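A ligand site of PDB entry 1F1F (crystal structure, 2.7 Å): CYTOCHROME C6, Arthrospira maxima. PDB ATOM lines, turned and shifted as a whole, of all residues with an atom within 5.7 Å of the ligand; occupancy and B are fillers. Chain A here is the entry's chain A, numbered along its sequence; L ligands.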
ATOM      1  N   VAL A   9     -26.047  -5.076 -14.197  1.00  0.00           N
ATOM      2  CA  VAL A   9     -25.032  -4.079 -13.883  1.00  0.00           C
ATOM      3  C   VAL A   9     -24.922  -3.987 -12.371  1.00  0.00           C
ATOM      4  O   VAL A   9     -23.836  -3.801 -11.822  1.00  0.00           O
ATOM      5  CB  VAL A   9     -25.424  -2.689 -14.439  1.00  0.00           C
ATOM      6  CG1 VAL A   9     -24.390  -1.647 -14.022  1.00  0.00           C
ATOM      7  CG2 VAL A   9     -25.542  -2.736 -15.952  1.00  0.00           C
ATOM      8  N   PHE A  10     -26.065  -4.128 -11.707  1.00  0.00           N
ATOM      9  CA  PHE A  10     -26.112  -4.052 -10.262  1.00  0.00           C
ATOM     10  C   PHE A  10     -25.399  -5.187  -9.552  1.00  0.00           C
ATOM     11  O   PHE A  10     -24.598  -4.951  -8.654  1.00  0.00           O
ATOM     12  CB  PHE A  10     -27.576  -3.982  -9.786  1.00  0.00           C
ATOM     13  CG  PHE A  10     -27.711  -3.818  -8.302  1.00  0.00           C
ATOM     14  CD1 PHE A  10     -27.820  -4.941  -7.469  1.00  0.00           C
ATOM     15  CD2 PHE A  10     -27.635  -2.561  -7.709  1.00  0.00           C
ATOM     16  CE1 PHE A  10     -27.848  -4.803  -6.085  1.00  0.00           C
ATOM     17  CE2 PHE A  10     -27.662  -2.412  -6.315  1.00  0.00           C
ATOM     18  CZ  PHE A  10     -27.772  -3.538  -5.514  1.00  0.00           C
ATOM     19  N   ASN A  13     -21.567  -4.913 -10.231  1.00  0.00           N
ATOM     20  CA  ASN A  13     -20.852  -3.759  -9.703  1.00  0.00           C
ATOM     21  C   ASN A  13     -21.342  -3.230  -8.364  1.00  0.00           C
ATOM     22  O   ASN A  13     -20.657  -2.417  -7.742  1.00  0.00           O
ATOM     23  CB  ASN A  13     -20.898  -2.587 -10.702  1.00  0.00           C
ATOM     24  CG  ASN A  13     -20.434  -2.954 -12.104  1.00  0.00           C
ATOM     25  OD1 ASN A  13     -21.220  -3.391 -12.944  1.00  0.00           O
ATOM     26  ND2 ASN A  13     -19.135  -2.784 -12.361  1.00  0.00           N
ATOM     27  N   CYS A  14     -22.501  -3.693  -7.894  1.00  0.00           N
ATOM     28  CA  CYS A  14     -23.053  -3.131  -6.657  1.00  0.00           C
ATOM     29  C   CYS A  14     -23.380  -4.072  -5.514  1.00  0.00           C
ATOM     30  O   CYS A  14     -23.266  -3.708  -4.346  1.00  0.00           O
ATOM     31  CB  CYS A  14     -24.312  -2.320  -6.990  1.00  0.00           C
ATOM     32  SG  CYS A  14     -24.303  -1.517  -8.610  1.00  0.00           S
ATOM     33  N   ALA A  16     -21.879  -6.304  -4.080  1.00  0.00           N
ATOM     34  CA  ALA A  16     -20.806  -6.476  -3.117  1.00  0.00           C
ATOM     35  C   ALA A  16     -21.016  -5.649  -1.860  1.00  0.00           C
ATOM     36  O   ALA A  16     -20.662  -6.067  -0.762  1.00  0.00           O
ATOM     37  CB  ALA A  16     -19.463  -6.083  -3.749  1.00  0.00           C
ATOM     38  N   CYS A  17     -21.595  -4.453  -2.027  1.00  0.00           N
ATOM     39  CA  CYS A  17     -21.842  -3.551  -0.904  1.00  0.00           C
ATOM     40  C   CYS A  17     -23.315  -3.288  -0.654  1.00  0.00           C
ATOM     41  O   CYS A  17     -23.697  -2.988   0.478  1.00  0.00           O
ATOM     42  CB  CYS A  17     -21.161  -2.208  -1.154  1.00  0.00           C
ATOM     43  SG  CYS A  17     -19.399  -2.259  -1.465  1.00  0.00           S
ATOM     44  N   HIS A  18     -24.137  -3.392  -1.683  1.00  0.00           N
ATOM     45  CA  HIS A  18     -25.556  -3.115  -1.536  1.00  0.00           C
ATOM     46  C   HIS A  18     -26.439  -4.366  -1.701  1.00  0.00           C
ATOM     47  O   HIS A  18     -27.547  -4.277  -2.229  1.00  0.00           O
ATOM     48  CB  HIS A  18     -25.984  -2.034  -2.540  1.00  0.00           C
ATOM     49  CG  HIS A  18     -25.316  -0.715  -2.340  1.00  0.00           C
ATOM     50  ND1 HIS A  18     -25.417   0.022  -1.179  1.00  0.00           N
ATOM     51  CD2 HIS A  18     -24.536   0.025  -3.169  1.00  0.00           C
ATOM     52  CE1 HIS A  18     -24.752   1.149  -1.303  1.00  0.00           C
ATOM     53  NE2 HIS A  18     -24.207   1.179  -2.506  1.00  0.00           N
ATOM     54  N   ASN A  23     -26.603  -1.442   2.905  1.00  0.00           N
ATOM     55  CA  ASN A  23     -25.323  -0.759   2.822  1.00  0.00           C
ATOM     56  C   ASN A  23     -24.375  -1.324   3.882  1.00  0.00           C
ATOM     57  O   ASN A  23     -24.296  -0.803   5.005  1.00  0.00           O
ATOM     58  CB  ASN A  23     -25.482   0.743   3.033  1.00  0.00           C
ATOM     59  CG  ASN A  23     -24.314   1.533   2.455  1.00  0.00           C
ATOM     60  OD1 ASN A  23     -23.151   1.155   2.634  1.00  0.00           O
ATOM     61  ND2 ASN A  23     -24.612   2.632   1.766  1.00  0.00           N
ATOM     62  N   ILE A  25     -21.329  -1.034   4.342  1.00  0.00           N
ATOM     63  CA  ILE A  25     -20.363  -0.085   4.864  1.00  0.00           C
ATOM     64  C   ILE A  25     -21.008   0.966   5.777  1.00  0.00           C
ATOM     65  O   ILE A  25     -20.601   1.110   6.933  1.00  0.00           O
ATOM     66  CB  ILE A  25     -19.610   0.656   3.726  1.00  0.00           C
ATOM     67  CG1 ILE A  25     -18.798  -0.340   2.887  1.00  0.00           C
ATOM     68  CG2 ILE A  25     -18.649   1.669   4.341  1.00  0.00           C
ATOM     69  CD1 ILE A  25     -19.619  -1.469   2.246  1.00  0.00           C
ATOM     70  N   VAL A  26     -21.982   1.712   5.259  1.00  0.00           N
ATOM     71  CA  VAL A  26     -22.661   2.732   6.060  1.00  0.00           C
ATOM     72  C   VAL A  26     -24.112   2.283   6.285  1.00  0.00           C
ATOM     73  O   VAL A  26     -25.017   2.550   5.484  1.00  0.00           O
ATOM     74  CB  VAL A  26     -22.616   4.125   5.353  1.00  0.00           C
ATOM     75  CG1 VAL A  26     -23.473   5.128   6.112  1.00  0.00           C
ATOM     76  CG2 VAL A  26     -21.178   4.627   5.295  1.00  0.00           C
ATOM     77  N   ASN A  28     -26.880   3.117   7.825  1.00  0.00           N
ATOM     78  CA  ASN A  28     -28.066   3.938   7.631  1.00  0.00           C
ATOM     79  C   ASN A  28     -28.239   4.582   6.243  1.00  0.00           C
ATOM     80  O   ASN A  28     -29.101   5.461   6.065  1.00  0.00           O
ATOM     81  CB  ASN A  28     -28.109   5.030   8.725  1.00  0.00           C
ATOM     82  CG  ASN A  28     -27.094   6.142   8.490  1.00  0.00           C
ATOM     83  OD1 ASN A  28     -25.980   5.895   7.995  1.00  0.00           O
ATOM     84  ND2 ASN A  28     -27.457   7.370   8.866  1.00  0.00           N
ATOM     85  N   LYS A  29     -27.423   4.158   5.275  1.00  0.00           N
ATOM     86  CA  LYS A  29     -27.498   4.685   3.910  1.00  0.00           C
ATOM     87  C   LYS A  29     -27.942   3.652   2.886  1.00  0.00           C
ATOM     88  O   LYS A  29     -27.285   3.457   1.851  1.00  0.00           O
ATOM     89  CB  LYS A  29     -26.143   5.254   3.480  1.00  0.00           C
ATOM     90  CG  LYS A  29     -25.773   6.535   4.172  1.00  0.00           C
ATOM     91  CD  LYS A  29     -26.685   7.696   3.768  1.00  0.00           C
ATOM     92  CE  LYS A  29     -26.177   8.986   4.395  1.00  0.00           C
ATOM     93  NZ  LYS A  29     -24.695   9.125   4.159  1.00  0.00           N
ATOM     94  N   THR A  30     -29.055   2.994   3.166  1.00  0.00           N
ATOM     95  CA  THR A  30     -29.581   1.952   2.289  1.00  0.00           C
ATOM     96  C   THR A  30     -30.182   2.479   0.994  1.00  0.00           C
ATOM     97  O   THR A  30     -30.278   3.692   0.772  1.00  0.00           O
ATOM     98  CB  THR A  30     -30.662   1.134   2.997  1.00  0.00           C
ATOM     99  OG1 THR A  30     -31.744   1.998   3.383  1.00  0.00           O
ATOM    100  CG2 THR A  30     -30.073   0.457   4.234  1.00  0.00           C
ATOM    101  N   LEU A  31     -30.587   1.555   0.130  1.00  0.00           N
ATOM    102  CA  LEU A  31     -31.197   1.918  -1.133  1.00  0.00           C
ATOM    103  C   LEU A  31     -32.708   1.712  -1.021  1.00  0.00           C
ATOM    104  O   LEU A  31     -33.370   1.264  -1.959  1.00  0.00           O
ATOM    105  CB  LEU A  31     -30.613   1.059  -2.255  1.00  0.00           C
ATOM    106  CG  LEU A  31     -29.070   1.012  -2.336  1.00  0.00           C
ATOM    107  CD1 LEU A  31     -28.653   0.043  -3.434  1.00  0.00           C
ATOM    108  CD2 LEU A  31     -28.494   2.401  -2.597  1.00  0.00           C
ATOM    109  N   SER A  32     -33.240   2.016   0.159  1.00  0.00           N
ATOM    110  CA  SER A  32     -34.673   1.903   0.405  1.00  0.00           C
ATOM    111  C   SER A  32     -35.291   3.219  -0.088  1.00  0.00           C
ATOM    112  O   SER A  32     -34.595   4.230  -0.210  1.00  0.00           O
ATOM    113  CB  SER A  32     -34.977   1.744   1.893  1.00  0.00           C
ATOM    114  OG  SER A  32     -34.916   2.994   2.580  1.00  0.00           O
ATOM    115  N   ASP A  35     -34.703   6.044   2.550  1.00  0.00           N
ATOM    116  CA  ASP A  35     -33.323   6.513   2.587  1.00  0.00           C
ATOM    117  C   ASP A  35     -32.952   7.302   1.351  1.00  0.00           C
ATOM    118  O   ASP A  35     -32.342   8.364   1.437  1.00  0.00           O
ATOM    119  CB  ASP A  35     -32.385   5.322   2.781  1.00  0.00           C
ATOM    120  CG  ASP A  35     -32.161   4.995   4.236  1.00  0.00           C
ATOM    121  OD1 ASP A  35     -33.020   5.389   5.058  1.00  0.00           O
ATOM    122  OD2 ASP A  35     -31.132   4.359   4.555  1.00  0.00           O
ATOM    123  N   LEU A  36     -33.315   6.780   0.181  1.00  0.00           N
ATOM    124  CA  LEU A  36     -33.050   7.466  -1.067  1.00  0.00           C
ATOM    125  C   LEU A  36     -33.726   8.844  -1.035  1.00  0.00           C
ATOM    126  O   LEU A  36     -33.201   9.821  -1.557  1.00  0.00           O
ATOM    127  CB  LEU A  36     -33.573   6.637  -2.245  1.00  0.00           C
ATOM    128  CG  LEU A  36     -32.545   5.912  -3.137  1.00  0.00           C
ATOM    129  CD1 LEU A  36     -31.169   5.786  -2.463  1.00  0.00           C
ATOM    130  CD2 LEU A  36     -33.110   4.531  -3.484  1.00  0.00           C
ATOM    131  N   TYR A  39     -31.772  11.096   1.909  1.00  0.00           N
ATOM    132  CA  TYR A  39     -30.412  11.544   1.569  1.00  0.00           C
ATOM    133  C   TYR A  39     -30.069  11.875   0.121  1.00  0.00           C
ATOM    134  O   TYR A  39     -29.110  12.611  -0.127  1.00  0.00           O
ATOM    135  CB  TYR A  39     -29.374  10.554   2.105  1.00  0.00           C
ATOM    136  CG  TYR A  39     -29.615  10.078   3.519  1.00  0.00           C
ATOM    137  CD1 TYR A  39     -30.146   8.808   3.758  1.00  0.00           C
ATOM    138  CD2 TYR A  39     -29.340  10.900   4.609  1.00  0.00           C
ATOM    139  CE1 TYR A  39     -30.419   8.374   5.057  1.00  0.00           C
ATOM    140  CE2 TYR A  39     -29.607  10.465   5.921  1.00  0.00           C
ATOM    141  CZ  TYR A  39     -30.150   9.209   6.143  1.00  0.00           C
ATOM    142  OH  TYR A  39     -30.468   8.789   7.425  1.00  0.00           O
ATOM    143  N   LEU A  40     -30.812  11.365  -0.861  1.00  0.00           N
ATOM    144  CA  LEU A  40     -30.473  11.682  -2.254  1.00  0.00           C
ATOM    145  C   LEU A  40     -31.042  12.995  -2.817  1.00  0.00           C
ATOM    146  O   LEU A  40     -32.252  13.105  -3.061  1.00  0.00           O
ATOM    147  CB  LEU A  40     -30.871  10.554  -3.212  1.00  0.00           C
ATOM    148  CG  LEU A  40     -29.758   9.619  -3.680  1.00  0.00           C
ATOM    149  CD1 LEU A  40     -30.253   8.840  -4.891  1.00  0.00           C
ATOM    150  CD2 LEU A  40     -28.527  10.415  -4.069  1.00  0.00           C
ATOM    151  N   VAL A  51     -30.296   9.079  -8.709  1.00  0.00           N
ATOM    152  CA  VAL A  51     -29.522   7.874  -8.478  1.00  0.00           C
ATOM    153  C   VAL A  51     -28.386   7.779  -9.491  1.00  0.00           C
ATOM    154  O   VAL A  51     -27.251   7.450  -9.139  1.00  0.00           O
ATOM    155  CB  VAL A  51     -30.408   6.620  -8.580  1.00  0.00           C
ATOM    156  CG1 VAL A  51     -29.554   5.373  -8.593  1.00  0.00           C
ATOM    157  CG2 VAL A  51     -31.349   6.577  -7.402  1.00  0.00           C
ATOM    158  N   GLN A  54     -25.435   9.986  -8.297  1.00  0.00           N
ATOM    159  CA  GLN A  54     -24.573   9.461  -7.242  1.00  0.00           C
ATOM    160  C   GLN A  54     -23.732   8.323  -7.806  1.00  0.00           C
ATOM    161  O   GLN A  54     -22.616   8.095  -7.353  1.00  0.00           O
ATOM    162  CB  GLN A  54     -25.413   8.957  -6.063  1.00  0.00           C
ATOM    163  CG  GLN A  54     -24.676   8.007  -5.118  1.00  0.00           C
ATOM    164  CD  GLN A  54     -24.245   8.669  -3.806  1.00  0.00           C
ATOM    165  OE1 GLN A  54     -23.562   8.045  -2.978  1.00  0.00           O
ATOM    166  NE2 GLN A  54     -24.642   9.944  -3.622  1.00  0.00           N
ATOM    167  N   VAL A  55     -24.275   7.606  -8.779  1.00  0.00           N
ATOM    168  CA  VAL A  55     -23.545   6.493  -9.383  1.00  0.00           C
ATOM    169  C   VAL A  55     -22.388   6.994 -10.226  1.00  0.00           C
ATOM    170  O   VAL A  55     -21.269   6.484 -10.129  1.00  0.00           O
ATOM    171  CB  VAL A  55     -24.482   5.605 -10.251  1.00  0.00           C
ATOM    172  CG1 VAL A  55     -23.668   4.708 -11.164  1.00  0.00           C
ATOM    173  CG2 VAL A  55     -25.354   4.734  -9.348  1.00  0.00           C
ATOM    174  N   LYS A  59     -19.437   9.288  -3.693  1.00  0.00           N
ATOM    175  CA  LYS A  59     -18.933  10.106  -2.594  1.00  0.00           C
ATOM    176  C   LYS A  59     -18.440   9.241  -1.433  1.00  0.00           C
ATOM    177  O   LYS A  59     -18.868   8.098  -1.274  1.00  0.00           O
ATOM    178  CB  LYS A  59     -20.008  11.064  -2.087  1.00  0.00           C
ATOM    179  CG  LYS A  59     -21.197  10.406  -1.435  1.00  0.00           C
ATOM    180  CD  LYS A  59     -22.209  11.474  -1.006  1.00  0.00           C
ATOM    181  CE  LYS A  59     -21.737  12.232   0.245  1.00  0.00           C
ATOM    182  NZ  LYS A  59     -21.898  11.390   1.473  1.00  0.00           N
ATOM    183  N   ASN A  60     -17.531   9.781  -0.629  1.00  0.00           N
ATOM    184  CA  ASN A  60     -16.986   9.056   0.508  1.00  0.00           C
ATOM    185  C   ASN A  60     -16.578   7.620   0.137  1.00  0.00           C
ATOM    186  O   ASN A  60     -15.777   7.410  -0.764  1.00  0.00           O
ATOM    187  CB  ASN A  60     -18.011   9.029   1.656  1.00  0.00           C
ATOM    188  CG  ASN A  60     -18.562  10.414   1.982  1.00  0.00           C
ATOM    189  OD1 ASN A  60     -17.888  11.423   1.768  1.00  0.00           O
ATOM    190  ND2 ASN A  60     -19.787  10.471   2.525  1.00  0.00           N
ATOM    191  N   ALA A  61     -17.136   6.640   0.830  1.00  0.00           N
ATOM    192  CA  ALA A  61     -16.793   5.250   0.579  1.00  0.00           C
ATOM    193  C   ALA A  61     -17.461   4.719  -0.675  1.00  0.00           C
ATOM    194  O   ALA A  61     -17.180   3.608  -1.123  1.00  0.00           O
ATOM    195  CB  ALA A  61     -17.166   4.384   1.787  1.00  0.00           C
ATOM    196  N   MET A  62     -18.371   5.513  -1.236  1.00  0.00           N
ATOM    197  CA  MET A  62     -19.080   5.138  -2.461  1.00  0.00           C
ATOM    198  C   MET A  62     -18.246   5.567  -3.657  1.00  0.00           C
ATOM    199  O   MET A  62     -18.061   6.766  -3.894  1.00  0.00           O
ATOM    200  CB  MET A  62     -20.442   5.821  -2.510  1.00  0.00           C
ATOM    201  CG  MET A  62     -21.113   5.834  -3.869  1.00  0.00           C
ATOM    202  SD  MET A  62     -21.879   4.292  -4.406  1.00  0.00           S
ATOM    203  CE  MET A  62     -22.318   4.732  -6.113  1.00  0.00           C
ATOM    204  N   PRO A  63     -17.711   4.601  -4.419  1.00  0.00           N
ATOM    205  CA  PRO A  63     -16.897   4.954  -5.595  1.00  0.00           C
ATOM    206  C   PRO A  63     -17.739   5.417  -6.781  1.00  0.00           C
ATOM    207  O   PRO A  63     -18.916   5.083  -6.889  1.00  0.00           O
ATOM    208  CB  PRO A  63     -16.144   3.651  -5.885  1.00  0.00           C
ATOM    209  CG  PRO A  63     -17.117   2.607  -5.470  1.00  0.00           C
ATOM    210  CD  PRO A  63     -17.667   3.154  -4.165  1.00  0.00           C
ATOM    211  N   PHE A  65     -18.462   5.627 -10.914  1.00  0.00           N
ATOM    212  CA  PHE A  65     -18.292   4.652 -11.981  1.00  0.00           C
ATOM    213  C   PHE A  65     -18.175   5.314 -13.356  1.00  0.00           C
ATOM    214  O   PHE A  65     -18.157   4.639 -14.396  1.00  0.00           O
ATOM    215  CB  PHE A  65     -19.446   3.633 -11.949  1.00  0.00           C
ATOM    216  CG  PHE A  65     -19.431   2.728 -10.738  1.00  0.00           C
ATOM    217  CD1 PHE A  65     -19.793   3.203  -9.487  1.00  0.00           C
ATOM    218  CD2 PHE A  65     -18.995   1.415 -10.848  1.00  0.00           C
ATOM    219  CE1 PHE A  65     -19.725   2.378  -8.350  1.00  0.00           C
ATOM    220  CE2 PHE A  65     -18.918   0.584  -9.740  1.00  0.00           C
ATOM    221  CZ  PHE A  65     -19.289   1.074  -8.484  1.00  0.00           C
ATOM    222  N   LEU A  69     -18.365   2.487 -16.104  1.00  0.00           N
ATOM    223  CA  LEU A  69     -19.671   2.193 -16.690  1.00  0.00           C
ATOM    224  C   LEU A  69     -20.028   3.187 -17.781  1.00  0.00           C
ATOM    225  O   LEU A  69     -19.617   4.355 -17.758  1.00  0.00           O
ATOM    226  CB  LEU A  69     -20.753   2.179 -15.616  1.00  0.00           C
ATOM    227  CG  LEU A  69     -21.198   0.830 -15.023  1.00  0.00           C
ATOM    228  CD1 LEU A  69     -20.171  -0.268 -15.281  1.00  0.00           C
ATOM    229  CD2 LEU A  69     -21.429   1.017 -13.531  1.00  0.00           C
ATOM    230  N   VAL A  77     -28.888   0.857 -14.384  1.00  0.00           N
ATOM    231  CA  VAL A  77     -28.767   0.400 -12.998  1.00  0.00           C
ATOM    232  C   VAL A  77     -29.596   1.332 -12.108  1.00  0.00           C
ATOM    233  O   VAL A  77     -30.140   0.924 -11.071  1.00  0.00           O
ATOM    234  CB  VAL A  77     -27.260   0.332 -12.563  1.00  0.00           C
ATOM    235  CG1 VAL A  77     -26.686   1.728 -12.344  1.00  0.00           C
ATOM    236  CG2 VAL A  77     -27.120  -0.517 -11.313  1.00  0.00           C
ATOM    237  N   VAL A  81     -32.543   0.273  -9.596  1.00  0.00           N
ATOM    238  CA  VAL A  81     -32.494   0.641  -8.193  1.00  0.00           C
ATOM    239  C   VAL A  81     -33.771   1.333  -7.757  1.00  0.00           C
ATOM    240  O   VAL A  81     -34.340   1.010  -6.703  1.00  0.00           O
ATOM    241  CB  VAL A  81     -31.288   1.567  -7.911  1.00  0.00           C
ATOM    242  CG1 VAL A  81     -31.537   2.388  -6.644  1.00  0.00           C
ATOM    243  CG2 VAL A  81     -30.042   0.734  -7.739  1.00  0.00           C
HETATM  244 FE1  LIG L   1     -23.269   2.679  -3.478  1.00  0.00          FE
HETATM  245  C1  LIG L   1     -24.453   5.071  -1.371  1.00  0.00           C
HETATM  246  C2  LIG L   1     -25.917   3.107  -5.569  1.00  0.00           C
HETATM  247  C3  LIG L   1     -21.774   0.523  -5.772  1.00  0.00           C
HETATM  248  C4  LIG L   1     -20.840   1.869  -1.184  1.00  0.00           C
HETATM  249  N1  LIG L   1     -24.881   3.810  -3.443  1.00  0.00           N
HETATM  250  C5  LIG L   1     -25.235   4.763  -2.494  1.00  0.00           C
HETATM  251  C6  LIG L   1     -26.479   5.500  -2.870  1.00  0.00           C
HETATM  252  C7  LIG L   1     -26.795   5.036  -4.145  1.00  0.00           C
HETATM  253  C8  LIG L   1     -25.847   3.931  -4.437  1.00  0.00           C
HETATM  254  C9  LIG L   1     -27.919   5.559  -5.069  1.00  0.00           C
HETATM  255  C10 LIG L   1     -27.298   6.444  -1.937  1.00  0.00           C
HETATM  256  C11 LIG L   1     -27.671   5.691  -0.666  1.00  0.00           C
HETATM  257  C12 LIG L   1     -28.458   6.503   0.338  1.00  0.00           C
HETATM  258  O1  LIG L   1     -27.954   7.535   0.824  1.00  0.00           O
HETATM  259  O2  LIG L   1     -29.596   6.115   0.670  1.00  0.00           O
HETATM  260  N2  LIG L   1     -23.776   1.892  -5.248  1.00  0.00           N
HETATM  261  C13 LIG L   1     -24.964   2.151  -5.955  1.00  0.00           C
HETATM  262  C14 LIG L   1     -24.972   1.430  -7.228  1.00  0.00           C
HETATM  263  C15 LIG L   1     -23.769   0.777  -7.320  1.00  0.00           C
HETATM  264  C16 LIG L   1     -23.030   1.047  -6.085  1.00  0.00           C
HETATM  265  C17 LIG L   1     -26.119   1.346  -8.235  1.00  0.00           C
HETATM  266  C18 LIG L   1     -23.333   0.015  -8.413  1.00  0.00           C
HETATM  267  C19 LIG L   1     -22.825   0.660  -9.544  1.00  0.00           C
HETATM  268  N3  LIG L   1     -21.626   1.497  -3.492  1.00  0.00           N
HETATM  269  C20 LIG L   1     -21.112   0.732  -4.559  1.00  0.00           C
HETATM  270  C21 LIG L   1     -19.946  -0.056  -4.111  1.00  0.00           C
HETATM  271  C22 LIG L   1     -19.842   0.131  -2.738  1.00  0.00           C
HETATM  272  C23 LIG L   1     -20.819   1.166  -2.398  1.00  0.00           C
HETATM  273  C24 LIG L   1     -18.934  -0.825  -4.967  1.00  0.00           C
HETATM  274  C25 LIG L   1     -18.949  -0.528  -1.847  1.00  0.00           C
HETATM  275  C26 LIG L   1     -17.613  -0.242  -1.872  1.00  0.00           C
HETATM  276  N4  LIG L   1     -22.760   3.331  -1.679  1.00  0.00           N
HETATM  277  C27 LIG L   1     -21.697   2.903  -0.869  1.00  0.00           C
HETATM  278  C28 LIG L   1     -21.571   3.763   0.294  1.00  0.00           C
HETATM  279  C29 LIG L   1     -22.583   4.672   0.212  1.00  0.00           C
HETATM  280  C30 LIG L   1     -23.313   4.402  -0.989  1.00  0.00           C
HETATM  281  C31 LIG L   1     -20.470   3.729   1.354  1.00  0.00           C
HETATM  282  C32 LIG L   1     -22.877   5.856   1.132  1.00  0.00           C
HETATM  283  C33 LIG L   1     -21.821   6.928   0.961  1.00  0.00           C
HETATM  284  C34 LIG L   1     -22.205   8.236   1.634  1.00  0.00           C
HETATM  285  O3  LIG L   1     -23.099   8.943   1.107  1.00  0.00           O
HETATM  286  O4  LIG L   1     -21.615   8.551   2.684  1.00  0.00           O
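Residues that only touch the ligand: Asn 23, Ala 61, Gln 54, Leu 31, Leu 36, Tyr 39, Asp 35, Asn 13, Val 55, Phe 65, Val 77, Val 51, Pro 63 and Ile 25. Hydrophobic or aromatic side chains within 4 Å of the ligand: His 18, Ile 25, Leu 31, Leu 36, Tyr 39, Val 51, Val 55, Ala 61, Met 62, Pro 63, Phe 65 and Val 77. 22 residues have an atom within 4 Å of the ligand: Asn 13, Cys 14, Cys 17, His 18, Asn 23, Ile 25, Lys 29, Thr 30, Leu 31, Asp 35, Leu 36, Tyr 39, Val 51, Gln 54, Val 55, Lys 59, Asn 60, Ala 61, Met 62, Pro 63, Phe 65 and Val 77.
The backbone NH of Phe 65 lies within hydrogen-bond range of the backbone carbonyl oxygen of Val 55. OG1 of Thr 30 sits at hydrogen-bond distance from OG of Ser 32, at 3.4 Å. The side-chain amide oxygen (OD1) of Asn 13 lies close to the backbone carbonyl oxygen (O) of Val 9 (2.9 Å). The side-chain hydroxyl (OG) of Ser 32 lies within hydrogen-bond range of the backbone NH (N) of Asp 35, 3.1 Å away. The side-chain hydroxyl (OG1) of Thr 30 is in hydrogen-bond range of the side-chain carboxylate (OD2) of Asp 35, at 2.7 Å. N of Val 26 sits at hydrogen-bond distance from OD1 of Asn 23, 2.9 Å away. OD1 of Asn 23 lies close to N of Ile 25, 3.3 Å away. The backbone carbonyl oxygen (O) of Lys 29 lies within hydrogen-bond range of the side-chain amide nitrogen (ND2) of Asn 23.
The side-chain sulfur (SD) of Met 62 is bound to an iron atom (FE1) of the ligand (2.3 Å). The backbone carbonyl oxygen (O) of Thr 30 sits close to an oxygen (O2) of the ligand, at 2.5 Å. NZ of Lys 29 is in salt-bridge range of O3 of the ligand, at 3.4 Å. NZ of Lys 59 is in salt-bridge range of O3 of the ligand, 2.8 Å away. An iron atom (FE1) of the ligand is bound by a ring nitrogen (NE2) of His 18. The side-chain sulfur of Cys 17 is covalently linked to a carbon (C25) of the ligand (1.8 Å). ND2 of Asn 60 sits at hydrogen-bond distance from O4 of the ligand (2.7 Å). A carbon (C18) of the ligand is covalently linked to the side-chain sulfur (SG) of Cys 14, 1.8 Å away.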
